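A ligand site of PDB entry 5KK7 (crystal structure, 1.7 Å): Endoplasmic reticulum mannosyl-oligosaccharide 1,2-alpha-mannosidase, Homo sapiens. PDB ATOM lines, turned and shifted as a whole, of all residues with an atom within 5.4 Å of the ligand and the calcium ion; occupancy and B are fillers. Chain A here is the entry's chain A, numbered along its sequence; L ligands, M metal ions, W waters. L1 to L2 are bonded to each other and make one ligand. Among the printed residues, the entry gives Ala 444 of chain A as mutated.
O4 of LIG L1 sits at hydrogen-bond distance from N of Arg 217 (2.8 Å). The side-chain carboxylate (OD1) of Asp 219 is in hydrogen-bond range of an oxygen (O3) of LIG L1 (2.6 Å). The guanidinium group (NH1) of Arg 353 lies within hydrogen-bond range of an oxygen (O5) of LG2 L2, 2.8 Å away. OE1 of Glu 355 lies within hydrogen-bond range of O5 of LG2 L2 (2.7 Å). OE2 of Glu 419 lies close to O2 of LG2 L2, at 2.6 Å. OE1 of Glu 445 sits at hydrogen-bond distance from O3 of LG2 L2, at 2.8 Å. The side-chain carboxylate (OE2) of Glu 153 lies within hydrogen-bond range of an oxygen (O5) of LIG L1 (2.7 Å).
The nearest printed residue that does not touch the calcium ion is Glu 419 (4.1 Å).
The side-chain carboxylate of Glu 86 lies within salt-bridge range of the guanidinium group of Arg 90, 2.9 Å away. The side-chain carboxylate of Glu 445 lies within salt-bridge range of the guanidinium group of Arg 90, at 3.6 Å. The backbone carbonyl oxygen (O) of Arg 217 sits at hydrogen-bond distance from the backbone NH (N) of Ala 152, 2.9 Å away.
Water W6 bridges OE1 of Glu 358 and OE1 of Glu 223. Water W7 bridges OE1 of Glu 419 (2.7 Å) and OE2 of Glu 358 (2.8 Å). Water W1 bridges an oxygen (O3) of LIG L1 (2.6 Å) and the side-chain hydroxyl (OG) of Ser 220 (2.8 Å). Water W2 lies within hydrogen-bond range of the side-chain carboxylate (OE1) of Glu 86, an oxygen (O3) of LG2 L2 and the guanidinium group (NH2) of Arg 90.
Residues that only touch the ligand: Phe 85, Ile 89, Arg 90, Ala 152, Ala 216, Leu 281, Pro 354 and Phe 415. Hydrophobic or aromatic side chains that line the ligand: Phe 85, Ile 89, Ala 152, Ala 216, Leu 281, Pro 354, Phe 415 and Ala 444. Along chain A the residues within 4 Å of the ligand span positions 85 to 445.
The calcium ion is bound by water W7 (2.3 Å). Water W4 is bound to the calcium ion, at 2.4 Å. The calcium ion is bound by water W3 (2.4 Å). O2 of LG2 L2 binds the calcium ion (2.4 Å). O of Ala 444 binds the calcium ion. O1 of LG2 L2 binds the calcium ion (2.5 Å). Water W6 is bound to the calcium ion (2.6 Å).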
ATOM      1  N   PHE A  85     -36.054  25.137 -11.148  1.00  0.00           N
ATOM      2  CA  PHE A  85     -35.122  24.013 -11.093  1.00  0.00           C
ATOM      3  C   PHE A  85     -34.953  23.505  -9.664  1.00  0.00           C
ATOM      4  O   PHE A  85     -35.042  22.290  -9.406  1.00  0.00           O
ATOM      5  CB  PHE A  85     -33.780  24.450 -11.718  1.00  0.00           C
ATOM      6  CG  PHE A  85     -32.595  23.622 -11.327  1.00  0.00           C
ATOM      7  CD1 PHE A  85     -32.402  22.376 -11.876  1.00  0.00           C
ATOM      8  CD2 PHE A  85     -31.667  24.119 -10.438  1.00  0.00           C
ATOM      9  CE1 PHE A  85     -31.329  21.621 -11.524  1.00  0.00           C
ATOM     10  CE2 PHE A  85     -30.578  23.373 -10.069  1.00  0.00           C
ATOM     11  CZ  PHE A  85     -30.399  22.124 -10.622  1.00  0.00           C
ATOM     12  N   GLU A  86     -34.681  24.396  -8.731  1.00  0.00           N
ATOM     13  CA  GLU A  86     -34.468  23.944  -7.360  1.00  0.00           C
ATOM     14  C   GLU A  86     -35.744  23.322  -6.794  1.00  0.00           C
ATOM     15  O   GLU A  86     -35.687  22.277  -6.114  1.00  0.00           O
ATOM     16  CB  GLU A  86     -33.988  25.105  -6.491  1.00  0.00           C
ATOM     17  CG  GLU A  86     -32.626  25.677  -6.891  1.00  0.00           C
ATOM     18  CD  GLU A  86     -31.450  24.864  -6.374  1.00  0.00           C
ATOM     19  OE1 GLU A  86     -30.306  25.318  -6.570  1.00  0.00           O
ATOM     20  OE2 GLU A  86     -31.647  23.799  -5.749  1.00  0.00           O
ATOM     21  N   ILE A  89     -36.078  19.714  -8.469  1.00  0.00           N
ATOM     22  CA  ILE A  89     -35.197  18.609  -8.106  1.00  0.00           C
ATOM     23  C   ILE A  89     -35.331  18.255  -6.643  1.00  0.00           C
ATOM     24  O   ILE A  89     -35.183  17.085  -6.267  1.00  0.00           O
ATOM     25  CB  ILE A  89     -33.730  18.903  -8.490  1.00  0.00           C
ATOM     26  CG1 ILE A  89     -33.117  20.078  -7.728  1.00  0.00           C
ATOM     27  CG2 ILE A  89     -33.657  19.175  -9.975  1.00  0.00           C
ATOM     28  CD1 ILE A  89     -31.555  20.066  -7.835  1.00  0.00           C
ATOM     29  N   ARG A  90     -35.545  19.245  -5.778  1.00  0.00           N
ATOM     30  CA  ARG A  90     -35.616  19.008  -4.343  1.00  0.00           C
ATOM     31  C   ARG A  90     -37.028  18.609  -3.898  1.00  0.00           C
ATOM     32  O   ARG A  90     -37.222  17.514  -3.362  1.00  0.00           O
ATOM     33  CB  ARG A  90     -35.150  20.246  -3.564  1.00  0.00           C
ATOM     34  CG  ARG A  90     -33.763  20.756  -3.987  1.00  0.00           C
ATOM     35  CD  ARG A  90     -33.034  21.435  -2.829  1.00  0.00           C
ATOM     36  NE  ARG A  90     -32.004  22.330  -3.313  1.00  0.00           N
ATOM     37  CZ  ARG A  90     -31.129  22.945  -2.534  1.00  0.00           C
ATOM     38  NH1 ARG A  90     -31.114  22.717  -1.227  1.00  0.00           N
ATOM     39  NH2 ARG A  90     -30.260  23.803  -3.056  1.00  0.00           N
ATOM     40  N   THR A 150     -31.128  29.600 -17.307  1.00  0.00           N
ATOM     41  CA  THR A 150     -29.900  28.827 -17.193  1.00  0.00           C
ATOM     42  C   THR A 150     -30.107  27.467 -17.857  1.00  0.00           C
ATOM     43  O   THR A 150     -31.109  26.788 -17.617  1.00  0.00           O
ATOM     44  CB  THR A 150     -29.494  28.665 -15.715  1.00  0.00           C
ATOM     45  OG1 THR A 150     -29.170  29.957 -15.152  1.00  0.00           O
ATOM     46  CG2 THR A 150     -28.307  27.747 -15.538  1.00  0.00           C
ATOM     47  N   ALA A 152     -28.688  24.470 -17.615  1.00  0.00           N
ATOM     48  CA  ALA A 152     -28.848  23.313 -16.739  1.00  0.00           C
ATOM     49  C   ALA A 152     -30.220  23.334 -16.054  1.00  0.00           C
ATOM     50  O   ALA A 152     -30.819  22.281 -15.819  1.00  0.00           O
ATOM     51  CB  ALA A 152     -27.733  23.286 -15.687  1.00  0.00           C
ATOM     52  N   GLU A 153     -30.725  24.524 -15.725  1.00  0.00           N
ATOM     53  CA  GLU A 153     -31.989  24.607 -14.999  1.00  0.00           C
ATOM     54  C   GLU A 153     -33.164  24.165 -15.854  1.00  0.00           C
ATOM     55  O   GLU A 153     -34.083  23.514 -15.360  1.00  0.00           O
ATOM     56  CB  GLU A 153     -32.190  26.028 -14.453  1.00  0.00           C
ATOM     57  CG  GLU A 153     -31.169  26.321 -13.364  1.00  0.00           C
ATOM     58  CD  GLU A 153     -31.438  27.615 -12.618  1.00  0.00           C
ATOM     59  OE1 GLU A 153     -32.497  28.242 -12.848  1.00  0.00           O
ATOM     60  OE2 GLU A 153     -30.570  27.969 -11.799  1.00  0.00           O
ATOM     61  N   GLY A 215     -19.306  22.636 -15.204  1.00  0.00           N
ATOM     62  CA  GLY A 215     -19.690  22.975 -13.840  1.00  0.00           C
ATOM     63  C   GLY A 215     -21.001  23.719 -13.814  1.00  0.00           C
ATOM     64  O   GLY A 215     -21.909  23.443 -14.605  1.00  0.00           O
ATOM     65  N   ALA A 216     -21.108  24.697 -12.907  1.00  0.00           N
ATOM     66  CA  ALA A 216     -22.394  25.346 -12.665  1.00  0.00           C
ATOM     67  C   ALA A 216     -22.973  25.925 -13.956  1.00  0.00           C
ATOM     68  O   ALA A 216     -22.267  26.534 -14.749  1.00  0.00           O
ATOM     69  CB  ALA A 216     -22.203  26.456 -11.627  1.00  0.00           C
ATOM     70  N   ARG A 217     -24.281  25.713 -14.139  1.00  0.00           N
ATOM     71  CA  ARG A 217     -25.144  26.220 -15.204  1.00  0.00           C
ATOM     72  C   ARG A 217     -25.197  25.289 -16.420  1.00  0.00           C
ATOM     73  O   ARG A 217     -26.043  25.498 -17.292  1.00  0.00           O
ATOM     74  CB  ARG A 217     -24.778  27.637 -15.699  1.00  0.00           C
ATOM     75  CG  ARG A 217     -24.684  28.691 -14.578  1.00  0.00           C
ATOM     76  CD  ARG A 217     -24.741  30.106 -15.122  1.00  0.00           C
ATOM     77  NE  ARG A 217     -24.469  31.076 -14.078  1.00  0.00           N
ATOM     78  CZ  ARG A 217     -23.361  31.827 -13.977  1.00  0.00           C
ATOM     79  NH1 ARG A 217     -22.372  31.742 -14.874  1.00  0.00           N
ATOM     80  NH2 ARG A 217     -23.249  32.671 -12.965  1.00  0.00           N
ATOM     81  N   ALA A 218     -24.322  24.278 -16.512  1.00  0.00           N
ATOM     82  CA  ALA A 218     -24.355  23.357 -17.644  1.00  0.00           C
ATOM     83  C   ALA A 218     -24.283  21.895 -17.217  1.00  0.00           C
ATOM     84  O   ALA A 218     -24.898  21.037 -17.855  1.00  0.00           O
ATOM     85  CB  ALA A 218     -23.218  23.703 -18.621  1.00  0.00           C
ATOM     86  N   ASP A 219     -23.613  21.607 -16.085  1.00  0.00           N
ATOM     87  CA  ASP A 219     -23.355  20.238 -15.659  1.00  0.00           C
ATOM     88  C   ASP A 219     -24.533  19.270 -15.819  1.00  0.00           C
ATOM     89  O   ASP A 219     -24.397  18.227 -16.475  1.00  0.00           O
ATOM     90  CB  ASP A 219     -22.888  20.260 -14.193  1.00  0.00           C
ATOM     91  CG  ASP A 219     -23.833  21.039 -13.267  1.00  0.00           C
ATOM     92  OD1 ASP A 219     -23.469  21.162 -12.101  1.00  0.00           O
ATOM     93  OD2 ASP A 219     -24.914  21.548 -13.704  1.00  0.00           O
ATOM     94  N   SER A 220     -25.696  19.567 -15.228  1.00  0.00           N
ATOM     95  CA  SER A 220     -26.703  18.512 -15.182  1.00  0.00           C
ATOM     96  C   SER A 220     -27.476  18.356 -16.496  1.00  0.00           C
ATOM     97  O   SER A 220     -28.222  17.394 -16.648  1.00  0.00           O
ATOM     98  CB  SER A 220     -27.673  18.725 -13.998  1.00  0.00           C
ATOM     99  OG  SER A 220     -28.168  20.061 -13.879  1.00  0.00           O
ATOM    100  N   GLU A 223     -25.888  15.123 -17.394  1.00  0.00           N
ATOM    101  CA  GLU A 223     -26.391  14.103 -16.485  1.00  0.00           C
ATOM    102  C   GLU A 223     -27.817  13.679 -16.863  1.00  0.00           C
ATOM    103  O   GLU A 223     -28.121  12.488 -16.910  1.00  0.00           O
ATOM    104  CB  GLU A 223     -26.320  14.658 -15.043  1.00  0.00           C
ATOM    105  CG  GLU A 223     -26.958  13.825 -13.964  1.00  0.00           C
ATOM    106  CD  GLU A 223     -27.065  14.611 -12.667  1.00  0.00           C
ATOM    107  OE1 GLU A 223     -27.640  14.053 -11.713  1.00  0.00           O
ATOM    108  OE2 GLU A 223     -26.544  15.772 -12.625  1.00  0.00           O
ATOM    109  N   LEU A 281     -18.716  20.780  -8.483  1.00  0.00           N
ATOM    110  CA  LEU A 281     -19.883  20.266  -9.203  1.00  0.00           C
ATOM    111  C   LEU A 281     -19.483  19.303 -10.305  1.00  0.00           C
ATOM    112  O   LEU A 281     -20.242  18.379 -10.618  1.00  0.00           O
ATOM    113  CB  LEU A 281     -20.673  21.431  -9.802  1.00  0.00           C
ATOM    114  CG  LEU A 281     -21.302  22.442  -8.843  1.00  0.00           C
ATOM    115  CD1 LEU A 281     -21.834  23.618  -9.642  1.00  0.00           C
ATOM    116  CD2 LEU A 281     -22.393  21.762  -8.046  1.00  0.00           C
ATOM    117  N   ARG A 353     -21.227  19.351   0.096  1.00  0.00           N
ATOM    118  CA  ARG A 353     -21.748  18.925  -1.188  1.00  0.00           C
ATOM    119  C   ARG A 353     -21.486  17.435  -1.459  1.00  0.00           C
ATOM    120  O   ARG A 353     -20.499  16.863  -0.997  1.00  0.00           O
ATOM    121  CB  ARG A 353     -21.139  19.748  -2.320  1.00  0.00           C
ATOM    122  CG  ARG A 353     -21.665  21.190  -2.434  1.00  0.00           C
ATOM    123  CD  ARG A 353     -21.270  21.832  -3.750  1.00  0.00           C
ATOM    124  NE  ARG A 353     -21.410  23.290  -3.783  1.00  0.00           N
ATOM    125  CZ  ARG A 353     -22.506  23.950  -4.167  1.00  0.00           C
ATOM    126  NH1 ARG A 353     -23.610  23.316  -4.558  1.00  0.00           N
ATOM    127  NH2 ARG A 353     -22.492  25.281  -4.167  1.00  0.00           N
ATOM    128  N   PRO A 354     -22.361  16.800  -2.268  1.00  0.00           N
ATOM    129  CA  PRO A 354     -22.364  15.343  -2.419  1.00  0.00           C
ATOM    130  C   PRO A 354     -21.585  14.785  -3.603  1.00  0.00           C
ATOM    131  O   PRO A 354     -21.477  13.561  -3.694  1.00  0.00           O
ATOM    132  CB  PRO A 354     -23.848  15.058  -2.626  1.00  0.00           C
ATOM    133  CG  PRO A 354     -24.272  16.212  -3.463  1.00  0.00           C
ATOM    134  CD  PRO A 354     -23.567  17.392  -2.873  1.00  0.00           C
ATOM    135  N   GLU A 355     -21.086  15.605  -4.521  1.00  0.00           N
ATOM    136  CA  GLU A 355     -20.757  15.070  -5.854  1.00  0.00           C
ATOM    137  C   GLU A 355     -19.641  14.015  -5.822  1.00  0.00           C
ATOM    138  O   GLU A 355     -19.674  13.048  -6.590  1.00  0.00           O
ATOM    139  CB  GLU A 355     -20.370  16.205  -6.807  1.00  0.00           C
ATOM    140  CG  GLU A 355     -21.538  17.059  -7.316  1.00  0.00           C
ATOM    141  CD  GLU A 355     -21.959  18.135  -6.323  1.00  0.00           C
ATOM    142  OE1 GLU A 355     -23.012  18.774  -6.536  1.00  0.00           O
ATOM    143  OE2 GLU A 355     -21.246  18.321  -5.334  1.00  0.00           O
ATOM    144  N   GLU A 358     -21.344  10.873  -4.341  1.00  0.00           N
ATOM    145  CA  GLU A 358     -22.233  10.433  -5.408  1.00  0.00           C
ATOM    146  C   GLU A 358     -21.498   9.563  -6.412  1.00  0.00           C
ATOM    147  O   GLU A 358     -21.938   8.449  -6.752  1.00  0.00           O
ATOM    148  CB  GLU A 358     -22.824  11.660  -6.106  1.00  0.00           C
ATOM    149  CG  GLU A 358     -23.687  11.368  -7.326  1.00  0.00           C
ATOM    150  CD  GLU A 358     -24.193  12.632  -7.985  1.00  0.00           C
ATOM    151  OE1 GLU A 358     -24.882  12.550  -9.014  1.00  0.00           O
ATOM    152  OE2 GLU A 358     -23.883  13.726  -7.453  1.00  0.00           O
ATOM    153  N   PHE A 415     -29.173  19.298   0.958  1.00  0.00           N
ATOM    154  CA  PHE A 415     -28.577  18.186   0.237  1.00  0.00           C
ATOM    155  C   PHE A 415     -27.568  17.399   1.060  1.00  0.00           C
ATOM    156  O   PHE A 415     -27.186  16.311   0.648  1.00  0.00           O
ATOM    157  CB  PHE A 415     -27.946  18.646  -1.091  1.00  0.00           C
ATOM    158  CG  PHE A 415     -27.065  19.843  -1.006  1.00  0.00           C
ATOM    159  CD1 PHE A 415     -25.818  19.752  -0.422  1.00  0.00           C
ATOM    160  CD2 PHE A 415     -27.461  21.046  -1.577  1.00  0.00           C
ATOM    161  CE1 PHE A 415     -24.976  20.843  -0.378  1.00  0.00           C
ATOM    162  CE2 PHE A 415     -26.639  22.165  -1.522  1.00  0.00           C
ATOM    163  CZ  PHE A 415     -25.385  22.063  -0.921  1.00  0.00           C
ATOM    164  N   GLU A 419     -28.699  14.045  -0.025  1.00  0.00           N
ATOM    165  CA  GLU A 419     -27.753  13.437  -0.954  1.00  0.00           C
ATOM    166  C   GLU A 419     -26.524  12.838  -0.283  1.00  0.00           C
ATOM    167  O   GLU A 419     -26.249  11.657  -0.476  1.00  0.00           O
ATOM    168  CB  GLU A 419     -27.281  14.476  -1.969  1.00  0.00           C
ATOM    169  CG  GLU A 419     -28.360  15.149  -2.740  1.00  0.00           C
ATOM    170  CD  GLU A 419     -27.834  15.762  -4.028  1.00  0.00           C
ATOM    171  OE1 GLU A 419     -27.243  14.987  -4.836  1.00  0.00           O
ATOM    172  OE2 GLU A 419     -28.018  16.972  -4.205  1.00  0.00           O
ATOM    173  N   ALA A 444     -31.351  14.779  -9.812  1.00  0.00           N
ATOM    174  CA  ALA A 444     -30.210  15.651  -9.523  1.00  0.00           C
ATOM    175  C   ALA A 444     -29.976  15.859  -8.032  1.00  0.00           C
ATOM    176  O   ALA A 444     -28.918  16.395  -7.668  1.00  0.00           O
ATOM    177  CB  ALA A 444     -30.418  17.012 -10.177  1.00  0.00           C
ATOM    178  N   GLU A 445     -30.933  15.490  -7.182  1.00  0.00           N
ATOM    179  CA  GLU A 445     -30.847  15.640  -5.725  1.00  0.00           C
ATOM    180  C   GLU A 445     -31.013  14.279  -5.047  1.00  0.00           C
ATOM    181  O   GLU A 445     -31.582  14.173  -3.954  1.00  0.00           O
ATOM    182  CB  GLU A 445     -31.900  16.649  -5.231  1.00  0.00           C
ATOM    183  CG  GLU A 445     -31.753  17.105  -3.789  1.00  0.00           C
ATOM    184  CD  GLU A 445     -31.107  18.473  -3.597  1.00  0.00           C
ATOM    185  OE1 GLU A 445     -30.688  19.055  -4.595  1.00  0.00           O
ATOM    186  OE2 GLU A 445     -31.037  18.964  -2.446  1.00  0.00           O
HETATM  187  S1  LIG L   1     -27.280  22.560  -8.436  1.00  0.00           S
HETATM  188  C1  LIG L   1     -25.727  23.471  -8.972  1.00  0.00           C
HETATM  189  C2  LIG L   1     -25.989  24.936  -8.701  1.00  0.00           C
HETATM  190  O1  LIG L   1     -24.795  25.626  -8.931  1.00  0.00           O
HETATM  191  C3  LIG L   1     -24.939  27.020  -8.707  1.00  0.00           C
HETATM  192  O2  LIG L   1     -27.038  25.472  -9.570  1.00  0.00           O
HETATM  193  C4  LIG L   1     -25.447  23.176 -10.397  1.00  0.00           C
HETATM  194  O3  LIG L   1     -25.444  21.707 -10.552  1.00  0.00           O
HETATM  195  C5  LIG L   1     -26.404  23.849 -11.338  1.00  0.00           C
HETATM  196  O4  LIG L   1     -25.814  23.860 -12.676  1.00  0.00           O
HETATM  197  C6  LIG L   1     -26.670  25.295 -10.976  1.00  0.00           C
HETATM  198  C7  LIG L   1     -27.839  25.801 -11.788  1.00  0.00           C
HETATM  199  O5  LIG L   1     -28.003  27.195 -11.544  1.00  0.00           O
HETATM  200  C1  LG2 L   2     -26.772  21.073  -7.499  1.00  0.00           C
HETATM  201  C2  LG2 L   2     -27.974  20.121  -7.447  1.00  0.00           C
HETATM  202  C3  LG2 L   2     -27.992  19.301  -6.211  1.00  0.00           C
HETATM  203  C4  LG2 L   2     -27.751  20.087  -4.987  1.00  0.00           C
HETATM  204  C5  LG2 L   2     -26.388  20.781  -4.973  1.00  0.00           C
HETATM  205  C6  LG2 L   2     -25.213  19.838  -4.807  1.00  0.00           C
HETATM  206  O1  LG2 L   2     -27.882  19.261  -8.602  1.00  0.00           O
HETATM  207  O2  LG2 L   2     -26.991  18.224  -6.269  1.00  0.00           O
HETATM  208  O3  LG2 L   2     -28.778  21.083  -4.912  1.00  0.00           O
HETATM  209  O4  LG2 L   2     -26.256  21.560  -6.211  1.00  0.00           O
HETATM  210  O5  LG2 L   2     -23.960  20.582  -4.810  1.00  0.00           O
HETATM  211 CA    CA M   1     -26.686  17.026  -8.328  1.00  0.00          CA
HETATM  212  O   HOH W   1     -27.404  20.147 -11.183  1.00  0.00           O
HETATM  213  O   HOH W   2     -28.484  23.819  -5.643  1.00  0.00           O
HETATM  214  O   HOH W   3     -27.052  17.378 -10.651  1.00  0.00           O
HETATM  215  O   HOH W   4     -24.757  18.382  -8.534  1.00  0.00           O
HETATM  216  O   HOH W   5     -26.346  29.423 -11.328  1.00  0.00           O
HETATM  217  O   HOH W   6     -26.607  14.638  -9.260  1.00  0.00           O
HETATM  218  O   HOH W   7     -25.527  15.894  -6.732  1.00  0.00           O
